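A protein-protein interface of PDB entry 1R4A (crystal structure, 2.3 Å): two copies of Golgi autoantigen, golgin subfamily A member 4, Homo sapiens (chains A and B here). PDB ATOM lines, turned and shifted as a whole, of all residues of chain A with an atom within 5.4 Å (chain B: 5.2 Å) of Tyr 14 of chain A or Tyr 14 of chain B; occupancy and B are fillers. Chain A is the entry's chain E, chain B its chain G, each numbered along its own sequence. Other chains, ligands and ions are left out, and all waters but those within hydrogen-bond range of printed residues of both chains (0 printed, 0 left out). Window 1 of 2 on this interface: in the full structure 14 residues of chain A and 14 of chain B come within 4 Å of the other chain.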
ATOM      1  N   VAL A  10     -21.796   4.526 -16.609  1.00  0.00           N
ATOM      2  CA  VAL A  10     -21.850   4.388 -15.157  1.00  0.00           C
ATOM      3  C   VAL A  10     -22.151   5.702 -14.433  1.00  0.00           C
ATOM      4  O   VAL A  10     -22.951   5.735 -13.490  1.00  0.00           O
ATOM      5  CB  VAL A  10     -20.522   3.821 -14.608  1.00  0.00           C
ATOM      6  CG1 VAL A  10     -20.566   3.799 -13.095  1.00  0.00           C
ATOM      7  CG2 VAL A  10     -20.288   2.409 -15.148  1.00  0.00           C
ATOM      8  N   LEU A  11     -21.498   6.776 -14.879  1.00  0.00           N
ATOM      9  CA  LEU A  11     -21.663   8.116 -14.299  1.00  0.00           C
ATOM     10  C   LEU A  11     -23.126   8.555 -14.425  1.00  0.00           C
ATOM     11  O   LEU A  11     -23.713   9.101 -13.487  1.00  0.00           O
ATOM     12  CB  LEU A  11     -20.739   9.094 -15.040  1.00  0.00           C
ATOM     13  CG  LEU A  11     -19.730  10.009 -14.335  1.00  0.00           C
ATOM     14  CD1 LEU A  11     -19.482   9.621 -12.895  1.00  0.00           C
ATOM     15  CD2 LEU A  11     -18.447   9.965 -15.134  1.00  0.00           C
ATOM     16  N   PHE A  12     -23.711   8.301 -15.592  1.00  0.00           N
ATOM     17  CA  PHE A  12     -25.104   8.647 -15.838  1.00  0.00           C
ATOM     18  C   PHE A  12     -26.011   8.016 -14.776  1.00  0.00           C
ATOM     19  O   PHE A  12     -26.813   8.701 -14.139  1.00  0.00           O
ATOM     20  CB  PHE A  12     -25.535   8.155 -17.222  1.00  0.00           C
ATOM     21  CG  PHE A  12     -26.974   8.447 -17.541  1.00  0.00           C
ATOM     22  CD1 PHE A  12     -27.398   9.749 -17.757  1.00  0.00           C
ATOM     23  CD2 PHE A  12     -27.910   7.424 -17.579  1.00  0.00           C
ATOM     24  CE1 PHE A  12     -28.743  10.026 -18.003  1.00  0.00           C
ATOM     25  CE2 PHE A  12     -29.261   7.692 -17.826  1.00  0.00           C
ATOM     26  CZ  PHE A  12     -29.675   8.993 -18.036  1.00  0.00           C
ATOM     27  N   GLU A  13     -25.886   6.702 -14.608  1.00  0.00           N
ATOM     28  CA  GLU A  13     -26.670   5.957 -13.627  1.00  0.00           C
ATOM     29  C   GLU A  13     -26.501   6.588 -12.237  1.00  0.00           C
ATOM     30  O   GLU A  13     -27.477   6.870 -11.539  1.00  0.00           O
ATOM     31  CB  GLU A  13     -26.207   4.490 -13.604  1.00  0.00           C
ATOM     32  CG  GLU A  13     -27.324   3.467 -13.694  1.00  0.00           C
ATOM     33  CD  GLU A  13     -28.239   3.681 -14.891  1.00  0.00           C
ATOM     34  OE1 GLU A  13     -27.780   3.570 -16.038  1.00  0.00           O
ATOM     35  OE2 GLU A  13     -29.430   3.969 -14.683  1.00  0.00           O
ATOM     36  N   TYR A  14     -25.251   6.805 -11.842  1.00  0.00           N
ATOM     37  CA  TYR A  14     -24.948   7.414 -10.553  1.00  0.00           C
ATOM     38  C   TYR A  14     -25.635   8.772 -10.419  1.00  0.00           C
ATOM     39  O   TYR A  14     -26.404   9.001  -9.491  1.00  0.00           O
ATOM     40  CB  TYR A  14     -23.443   7.606 -10.415  1.00  0.00           C
ATOM     41  CG  TYR A  14     -23.016   8.247  -9.120  1.00  0.00           C
ATOM     42  CD1 TYR A  14     -23.052   7.535  -7.923  1.00  0.00           C
ATOM     43  CD2 TYR A  14     -22.554   9.566  -9.087  1.00  0.00           C
ATOM     44  CE1 TYR A  14     -22.634   8.116  -6.713  1.00  0.00           C
ATOM     45  CE2 TYR A  14     -22.138  10.158  -7.896  1.00  0.00           C
ATOM     46  CZ  TYR A  14     -22.180   9.426  -6.718  1.00  0.00           C
ATOM     47  OH  TYR A  14     -21.755   9.998  -5.528  1.00  0.00           O
ATOM     48  N   MET A  15     -25.358   9.666 -11.359  1.00  0.00           N
ATOM     49  CA  MET A  15     -25.933  11.006 -11.330  1.00  0.00           C
ATOM     50  C   MET A  15     -27.460  11.031 -11.361  1.00  0.00           C
ATOM     51  O   MET A  15     -28.077  12.037 -10.989  1.00  0.00           O
ATOM     52  CB  MET A  15     -25.353  11.845 -12.481  1.00  0.00           C
ATOM     53  CG  MET A  15     -23.835  11.962 -12.412  1.00  0.00           C
ATOM     54  SD  MET A  15     -23.124  13.216 -13.487  1.00  0.00           S
ATOM     55  CE  MET A  15     -22.763  12.262 -14.915  1.00  0.00           C
ATOM     56  N   MET A  16     -28.070   9.934 -11.803  1.00  0.00           N
ATOM     57  CA  MET A  16     -29.526   9.851 -11.842  1.00  0.00           C
ATOM     58  C   MET A  16     -30.073   9.229 -10.549  1.00  0.00           C
ATOM     59  O   MET A  16     -31.274   8.962 -10.443  1.00  0.00           O
ATOM     60  CB  MET A  16     -29.994   9.050 -13.062  1.00  0.00           C
ATOM     61  CG  MET A  16     -29.865   9.812 -14.387  1.00  0.00           C
ATOM     62  SD  MET A  16     -30.659  11.456 -14.386  1.00  0.00           S
ATOM     63  CE  MET A  16     -32.313  11.034 -14.060  1.00  0.00           C
ATOM     64  N   GLY A  17     -29.182   9.015  -9.581  1.00  0.00           N
ATOM     65  CA  GLY A  17     -29.570   8.448  -8.299  1.00  0.00           C
ATOM     66  C   GLY A  17     -29.864   6.952  -8.242  1.00  0.00           C
ATOM     67  O   GLY A  17     -30.490   6.493  -7.281  1.00  0.00           O
ATOM     68  N   ARG A  18     -29.416   6.189  -9.244  1.00  0.00           N
ATOM     69  CA  ARG A  18     -29.652   4.737  -9.286  1.00  0.00           C
ATOM     70  C   ARG A  18     -28.465   3.870  -8.841  1.00  0.00           C
ATOM     71  O   ARG A  18     -27.387   3.916  -9.435  1.00  0.00           O
ATOM     72  CB  ARG A  18     -30.061   4.314 -10.705  1.00  0.00           C
ATOM     73  CG  ARG A  18     -31.353   4.949 -11.217  1.00  0.00           C
ATOM     74  CD  ARG A  18     -31.519   4.744 -12.728  1.00  0.00           C
ATOM     75  NE  ARG A  18     -32.438   5.722 -13.313  1.00  0.00           N
ATOM     76  CZ  ARG A  18     -32.264   6.288 -14.506  1.00  0.00           C
ATOM     77  NH1 ARG A  18     -33.148   7.170 -14.966  1.00  0.00           N
ATOM     78  NH2 ARG A  18     -31.201   5.980 -15.234  1.00  0.00           N
ATOM     79  N   THR A  20     -26.457   4.137  -6.441  1.00  0.00           N
ATOM     80  CA  THR A  20     -25.321   5.013  -6.179  1.00  0.00           C
ATOM     81  C   THR A  20     -24.104   4.377  -5.504  1.00  0.00           C
ATOM     82  O   THR A  20     -22.970   4.636  -5.901  1.00  0.00           O
ATOM     83  CB  THR A  20     -25.769   6.261  -5.366  1.00  0.00           C
ATOM     84  OG1 THR A  20     -26.142   5.869  -4.037  1.00  0.00           O
ATOM     85  CG2 THR A  20     -26.966   6.941  -6.050  1.00  0.00           C
ATOM     86  N   LYS A  21     -24.326   3.539  -4.498  1.00  0.00           N
ATOM     87  CA  LYS A  21     -23.218   2.913  -3.783  1.00  0.00           C
ATOM     88  C   LYS A  21     -22.367   2.000  -4.667  1.00  0.00           C
ATOM     89  O   LYS A  21     -21.148   1.975  -4.522  1.00  0.00           O
ATOM     90  CB  LYS A  21     -23.742   2.133  -2.569  1.00  0.00           C
ATOM     91  CG  LYS A  21     -22.672   1.400  -1.778  1.00  0.00           C
ATOM     92  CD  LYS A  21     -21.634   2.369  -1.212  1.00  0.00           C
ATOM     93  CE  LYS A  21     -20.512   1.639  -0.466  1.00  0.00           C
ATOM     94  NZ  LYS A  21     -20.973   0.818   0.695  1.00  0.00           N
ATOM     95  N   MET A  23     -22.201   2.191  -8.096  1.00  0.00           N
ATOM     96  CA  MET A  23     -21.606   3.087  -9.088  1.00  0.00           C
ATOM     97  C   MET A  23     -20.388   3.792  -8.509  1.00  0.00           C
ATOM     98  O   MET A  23     -19.348   3.881  -9.163  1.00  0.00           O
ATOM     99  CB  MET A  23     -22.644   4.106  -9.562  1.00  0.00           C
ATOM    100  CG  MET A  23     -23.822   3.470 -10.312  1.00  0.00           C
ATOM    101  SD  MET A  23     -23.324   2.422 -11.714  1.00  0.00           S
ATOM    102  CE  MET A  23     -23.543   0.719 -11.044  1.00  0.00           C
ATOM    103  N   ALA A  24     -20.513   4.264  -7.273  1.00  0.00           N
ATOM    104  CA  ALA A  24     -19.417   4.951  -6.596  1.00  0.00           C
ATOM    105  C   ALA A  24     -18.175   4.086  -6.584  1.00  0.00           C
ATOM    106  O   ALA A  24     -17.058   4.565  -6.800  1.00  0.00           O
ATOM    107  CB  ALA A  24     -19.819   5.293  -5.170  1.00  0.00           C
ATOM    108  N   ILE A  27     -16.731   3.955 -10.307  1.00  0.00           N
ATOM    109  CA  ILE A  27     -16.189   5.241 -10.756  1.00  0.00           C
ATOM    110  C   ILE A  27     -14.798   5.476 -10.159  1.00  0.00           C
ATOM    111  O   ILE A  27     -13.845   5.775 -10.883  1.00  0.00           O
ATOM    112  CB  ILE A  27     -17.118   6.410 -10.361  1.00  0.00           C
ATOM    113  CG1 ILE A  27     -18.396   6.351 -11.193  1.00  0.00           C
ATOM    114  CG2 ILE A  27     -16.395   7.756 -10.580  1.00  0.00           C
ATOM    115  CD1 ILE A  27     -19.527   7.188 -10.651  1.00  0.00           C
ATOM    116  N   ILE A  41     -15.430   9.197   0.130  1.00  0.00           N
ATOM    117  CA  ILE A  41     -16.613   9.077  -0.719  1.00  0.00           C
ATOM    118  C   ILE A  41     -17.490   7.901  -0.270  1.00  0.00           C
ATOM    119  O   ILE A  41     -18.693   8.059  -0.075  1.00  0.00           O
ATOM    120  CB  ILE A  41     -16.200   8.869  -2.200  1.00  0.00           C
ATOM    121  CG1 ILE A  41     -15.467  10.108  -2.718  1.00  0.00           C
ATOM    122  CG2 ILE A  41     -17.421   8.565  -3.057  1.00  0.00           C
ATOM    123  CD1 ILE A  41     -14.960   9.981  -4.145  1.00  0.00           C
ATOM    124  N   GLU A  45     -21.404   7.832   1.256  1.00  0.00           N
ATOM    125  CA  GLU A  45     -22.301   7.005   0.469  1.00  0.00           C
ATOM    126  C   GLU A  45     -23.046   6.065   1.417  1.00  0.00           C
ATOM    127  O   GLU A  45     -24.259   5.907   1.308  1.00  0.00           O
ATOM    128  CB  GLU A  45     -21.496   6.221  -0.564  1.00  0.00           C
ATOM    129  CG  GLU A  45     -22.338   5.515  -1.590  1.00  0.00           C
ATOM    130  CD  GLU A  45     -23.321   6.433  -2.282  1.00  0.00           C
ATOM    131  OE1 GLU A  45     -22.886   7.424  -2.910  1.00  0.00           O
ATOM    132  OE2 GLU A  45     -24.533   6.156  -2.197  1.00  0.00           O
ATOM    133  N   VAL B  10     -13.151  17.745 -10.544  1.00  0.00           N
ATOM    134  CA  VAL B  10     -14.568  18.095 -10.588  1.00  0.00           C
ATOM    135  C   VAL B  10     -15.494  16.938 -10.166  1.00  0.00           C
ATOM    136  O   VAL B  10     -16.603  17.166  -9.671  1.00  0.00           O
ATOM    137  CB  VAL B  10     -14.961  18.584 -12.016  1.00  0.00           C
ATOM    138  CG1 VAL B  10     -16.461  18.736 -12.116  1.00  0.00           C
ATOM    139  CG2 VAL B  10     -14.295  19.941 -12.314  1.00  0.00           C
ATOM    140  N   LEU B  11     -15.036  15.704 -10.369  1.00  0.00           N
ATOM    141  CA  LEU B  11     -15.823  14.535 -10.002  1.00  0.00           C
ATOM    142  C   LEU B  11     -15.835  14.386  -8.479  1.00  0.00           C
ATOM    143  O   LEU B  11     -16.875  14.133  -7.878  1.00  0.00           O
ATOM    144  CB  LEU B  11     -15.240  13.282 -10.661  1.00  0.00           C
ATOM    145  CG  LEU B  11     -16.238  12.283 -11.267  1.00  0.00           C
ATOM    146  CD1 LEU B  11     -17.601  12.914 -11.456  1.00  0.00           C
ATOM    147  CD2 LEU B  11     -15.695  11.806 -12.613  1.00  0.00           C
ATOM    148  N   PHE B  12     -14.671  14.578  -7.868  1.00  0.00           N
ATOM    149  CA  PHE B  12     -14.533  14.491  -6.420  1.00  0.00           C
ATOM    150  C   PHE B  12     -15.479  15.453  -5.718  1.00  0.00           C
ATOM    151  O   PHE B  12     -16.232  15.068  -4.820  1.00  0.00           O
ATOM    152  CB  PHE B  12     -13.110  14.829  -6.004  1.00  0.00           C
ATOM    153  CG  PHE B  12     -12.892  14.757  -4.522  1.00  0.00           C
ATOM    154  CD1 PHE B  12     -12.859  13.522  -3.870  1.00  0.00           C
ATOM    155  CD2 PHE B  12     -12.765  15.922  -3.764  1.00  0.00           C
ATOM    156  CE1 PHE B  12     -12.704  13.453  -2.487  1.00  0.00           C
ATOM    157  CE2 PHE B  12     -12.612  15.860  -2.381  1.00  0.00           C
ATOM    158  CZ  PHE B  12     -12.581  14.630  -1.740  1.00  0.00           C
ATOM    159  N   GLU B  13     -15.420  16.709  -6.139  1.00  0.00           N
ATOM    160  CA  GLU B  13     -16.244  17.777  -5.594  1.00  0.00           C
ATOM    161  C   GLU B  13     -17.729  17.420  -5.675  1.00  0.00           C
ATOM    162  O   GLU B  13     -18.485  17.598  -4.715  1.00  0.00           O
ATOM    163  CB  GLU B  13     -15.959  19.061  -6.392  1.00  0.00           C
ATOM    164  CG  GLU B  13     -15.756  20.321  -5.559  1.00  0.00           C
ATOM    165  CD  GLU B  13     -14.815  20.115  -4.380  1.00  0.00           C
ATOM    166  OE1 GLU B  13     -13.700  19.587  -4.572  1.00  0.00           O
ATOM    167  OE2 GLU B  13     -15.196  20.495  -3.256  1.00  0.00           O
ATOM    168  N   TYR B  14     -18.136  16.912  -6.833  1.00  0.00           N
ATOM    169  CA  TYR B  14     -19.519  16.523  -7.073  1.00  0.00           C
ATOM    170  C   TYR B  14     -19.983  15.400  -6.129  1.00  0.00           C
ATOM    171  O   TYR B  14     -21.060  15.474  -5.537  1.00  0.00           O
ATOM    172  CB  TYR B  14     -19.667  16.060  -8.526  1.00  0.00           C
ATOM    173  CG  TYR B  14     -21.044  15.567  -8.862  1.00  0.00           C
ATOM    174  CD1 TYR B  14     -22.081  16.458  -9.086  1.00  0.00           C
ATOM    175  CD2 TYR B  14     -21.327  14.207  -8.903  1.00  0.00           C
ATOM    176  CE1 TYR B  14     -23.372  16.015  -9.343  1.00  0.00           C
ATOM    177  CE2 TYR B  14     -22.618  13.751  -9.157  1.00  0.00           C
ATOM    178  CZ  TYR B  14     -23.631  14.665  -9.374  1.00  0.00           C
ATOM    179  OH  TYR B  14     -24.909  14.238  -9.605  1.00  0.00           O
ATOM    180  N   MET B  15     -19.160  14.365  -5.999  1.00  0.00           N
ATOM    181  CA  MET B  15     -19.487  13.231  -5.155  1.00  0.00           C
ATOM    182  C   MET B  15     -19.409  13.522  -3.650  1.00  0.00           C
ATOM    183  O   MET B  15     -19.814  12.686  -2.839  1.00  0.00           O
ATOM    184  CB  MET B  15     -18.597  12.028  -5.507  1.00  0.00           C
ATOM    185  CG  MET B  15     -18.791  11.528  -6.944  1.00  0.00           C
ATOM    186  SD  MET B  15     -17.842  10.041  -7.388  1.00  0.00           S
ATOM    187  CE  MET B  15     -16.370  10.721  -8.008  1.00  0.00           C
ATOM    188  N   MET B  16     -18.891  14.692  -3.275  1.00  0.00           N
ATOM    189  CA  MET B  16     -18.833  15.054  -1.859  1.00  0.00           C
ATOM    190  C   MET B  16     -19.988  15.999  -1.554  1.00  0.00           C
ATOM    191  O   MET B  16     -20.105  16.529  -0.448  1.00  0.00           O
ATOM    192  CB  MET B  16     -17.493  15.699  -1.497  1.00  0.00           C
ATOM    193  CG  MET B  16     -16.314  14.713  -1.478  1.00  0.00           C
ATOM    194  SD  MET B  16     -16.526  13.282  -0.339  1.00  0.00           S
ATOM    195  CE  MET B  16     -16.473  14.109   1.255  1.00  0.00           C
ATOM    196  N   GLY B  17     -20.841  16.197  -2.558  1.00  0.00           N
ATOM    197  CA  GLY B  17     -22.023  17.029  -2.410  1.00  0.00           C
ATOM    198  C   GLY B  17     -21.901  18.540  -2.437  1.00  0.00           C
ATOM    199  O   GLY B  17     -22.807  19.227  -1.973  1.00  0.00           O
ATOM    200  N   ARG B  18     -20.811  19.073  -2.975  1.00  0.00           N
ATOM    201  CA  ARG B  18     -20.641  20.530  -3.025  1.00  0.00           C
ATOM    202  C   ARG B  18     -20.815  21.108  -4.445  1.00  0.00           C
ATOM    203  O   ARG B  18     -20.238  20.605  -5.403  1.00  0.00           O
ATOM    204  CB  ARG B  18     -19.248  20.920  -2.532  1.00  0.00           C
ATOM    205  CG  ARG B  18     -18.881  20.365  -1.170  1.00  0.00           C
ATOM    206  CD  ARG B  18     -17.377  20.448  -1.017  1.00  0.00           C
ATOM    207  NE  ARG B  18     -16.883  19.592   0.055  1.00  0.00           N
ATOM    208  CZ  ARG B  18     -15.779  18.859  -0.033  1.00  0.00           C
ATOM    209  NH1 ARG B  18     -15.398  18.106   0.990  1.00  0.00           N
ATOM    210  NH2 ARG B  18     -15.060  18.867  -1.157  1.00  0.00           N
ATOM    211  N   THR B  20     -23.033  20.810  -6.609  1.00  0.00           N
ATOM    212  CA  THR B  20     -23.378  19.709  -7.506  1.00  0.00           C
ATOM    213  C   THR B  20     -23.964  20.086  -8.871  1.00  0.00           C
ATOM    214  O   THR B  20     -23.664  19.435  -9.871  1.00  0.00           O
ATOM    215  CB  THR B  20     -24.328  18.688  -6.787  1.00  0.00           C
ATOM    216  OG1 THR B  20     -25.579  19.314  -6.480  1.00  0.00           O
ATOM    217  CG2 THR B  20     -23.695  18.191  -5.467  1.00  0.00           C
ATOM    218  N   MET B  23     -20.981  21.388 -11.098  1.00  0.00           N
ATOM    219  CA  MET B  23     -20.090  20.273 -11.398  1.00  0.00           C
ATOM    220  C   MET B  23     -20.766  19.367 -12.440  1.00  0.00           C
ATOM    221  O   MET B  23     -20.102  18.819 -13.313  1.00  0.00           O
ATOM    222  CB  MET B  23     -19.781  19.473 -10.122  1.00  0.00           C
ATOM    223  CG  MET B  23     -19.070  20.268  -9.030  1.00  0.00           C
ATOM    224  SD  MET B  23     -17.423  20.850  -9.525  1.00  0.00           S
ATOM    225  CE  MET B  23     -17.767  22.604  -9.932  1.00  0.00           C
ATOM    226  N   ALA B  24     -22.085  19.225 -12.354  1.00  0.00           N
ATOM    227  CA  ALA B  24     -22.821  18.379 -13.300  1.00  0.00           C
ATOM    228  C   ALA B  24     -22.671  18.888 -14.730  1.00  0.00           C
ATOM    229  O   ALA B  24     -22.562  18.105 -15.672  1.00  0.00           O
ATOM    230  CB  ALA B  24     -24.309  18.312 -12.913  1.00  0.00           C
ATOM    231  N   ILE B  27     -18.996  18.160 -15.987  1.00  0.00           N
ATOM    232  CA  ILE B  27     -18.782  16.720 -16.172  1.00  0.00           C
ATOM    233  C   ILE B  27     -19.371  16.206 -17.497  1.00  0.00           C
ATOM    234  O   ILE B  27     -18.696  15.507 -18.253  1.00  0.00           O
ATOM    235  CB  ILE B  27     -19.383  15.896 -14.993  1.00  0.00           C
ATOM    236  CG1 ILE B  27     -18.549  16.117 -13.728  1.00  0.00           C
ATOM    237  CG2 ILE B  27     -19.400  14.409 -15.347  1.00  0.00           C
ATOM    238  CD1 ILE B  27     -19.155  15.566 -12.475  1.00  0.00           C
ATOM    239  N   ILE B  41     -30.065  14.552 -16.502  1.00  0.00           N
ATOM    240  CA  ILE B  41     -29.316  14.851 -15.278  1.00  0.00           C
ATOM    241  C   ILE B  41     -29.579  16.288 -14.821  1.00  0.00           C
ATOM    242  O   ILE B  41     -29.721  16.560 -13.628  1.00  0.00           O
ATOM    243  CB  ILE B  41     -27.805  14.667 -15.506  1.00  0.00           C
ATOM    244  CG1 ILE B  41     -27.520  13.226 -15.946  1.00  0.00           C
ATOM    245  CG2 ILE B  41     -27.033  15.033 -14.238  1.00  0.00           C
ATOM    246  CD1 ILE B  41     -26.076  12.974 -16.347  1.00  0.00           C
ATOM    247  N   GLU B  45     -31.071  17.686 -11.007  1.00  0.00           N
ATOM    248  CA  GLU B  45     -30.226  18.624 -10.286  1.00  0.00           C
ATOM    249  C   GLU B  45     -31.070  19.859  -9.924  1.00  0.00           C
ATOM    250  O   GLU B  45     -30.945  20.409  -8.821  1.00  0.00           O
ATOM    251  CB  GLU B  45     -29.035  19.008 -11.161  1.00  0.00           C
ATOM    252  CG  GLU B  45     -27.843  19.490 -10.391  1.00  0.00           C
ATOM    253  CD  GLU B  45     -27.316  18.468  -9.404  1.00  0.00           C
ATOM    254  OE1 GLU B  45     -27.137  17.293  -9.785  1.00  0.00           O
ATOM    255  OE2 GLU B  45     -27.062  18.845  -8.242  1.00  0.00           O
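Among the printed residues, merely in contact across the chains: Phe 12 of chain A with Ile 41 of chain B (3.8 Å), Tyr 14 of chain A with Tyr 14 of chain B (3.8 Å), Tyr 14 of chain A with Met 15 of chain B (3.6 Å), Met 15 of chain A with Tyr 14 of chain B (3.8 Å), Met 15 of chain A with Ile 41 of chain B (3.7 Å) and Ile 27 of chain A with Met 15 of chain B (3.9 Å).
The side-chain sulfur (SD) of Met 16 of chain A lies close to the backbone NH (N) of Ile 41 of chain B (3.8 Å).
Of the printed residues of chain B, Phe 12 of chain A touches Ile 41.
Tyr 14 of chain A touches just these residues of chain B: Tyr 14 and Met 15.
Printed residues of chain B within 4 Å of Met 15 of chain A: Tyr 14 and Ile 41.
Printed residues of chain B within 4 Å of Met 16 of chain A: Ile 41 (3.8 Å).
Of the printed residues of chain A, Tyr 14 of chain B touches Tyr 14 (3.8 Å) and Met 15 (3.8 Å).
Of the printed residues of chain A, Met 15 of chain B touches Tyr 14 and Ile 27.
Ile 27 of chain B touches none of the printed residues of chain A.
Printed residues of chain A within 4 Å of Ile 41 of chain B: Phe 12 (3.8 Å), Met 15 (3.7 Å) and Met 16 (3.8 Å).
The nearest printed residue of chain B that does not touch Tyr 14 of chain A is Met 16 of chain B (5.9 Å).
The nearest printed residue of chain B that does not touch Ile 27 of chain A is Leu 11 of chain B (4.6 Å).
Printed residues of chain A that touch a printed residue of chain B: Phe 12, Tyr 14, Met 15, Met 16 and Ile 27.
Of the 15 printed residues of chain B, 3 touch a printed residue of chain A.
Tyr 14 of chain A touches its own counterpart, Tyr 14 of chain B.
Tyr 14 of chain A touches Met 15 of chain B, and with the chains exchanged Met 15 of chain A touches Tyr 14 of chain B.
Met 15 of chain A touches Ile 41 of chain B, but with the chains exchanged Ile 41 of chain A does not touch Met 15 of chain B (4.2 Å).
Ile 27 of chain A touches Met 15 of chain B, but with the chains exchanged Met 15 of chain A does not touch Ile 27 of chain B (4.01 Å).
15 positions are printed for both chains.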
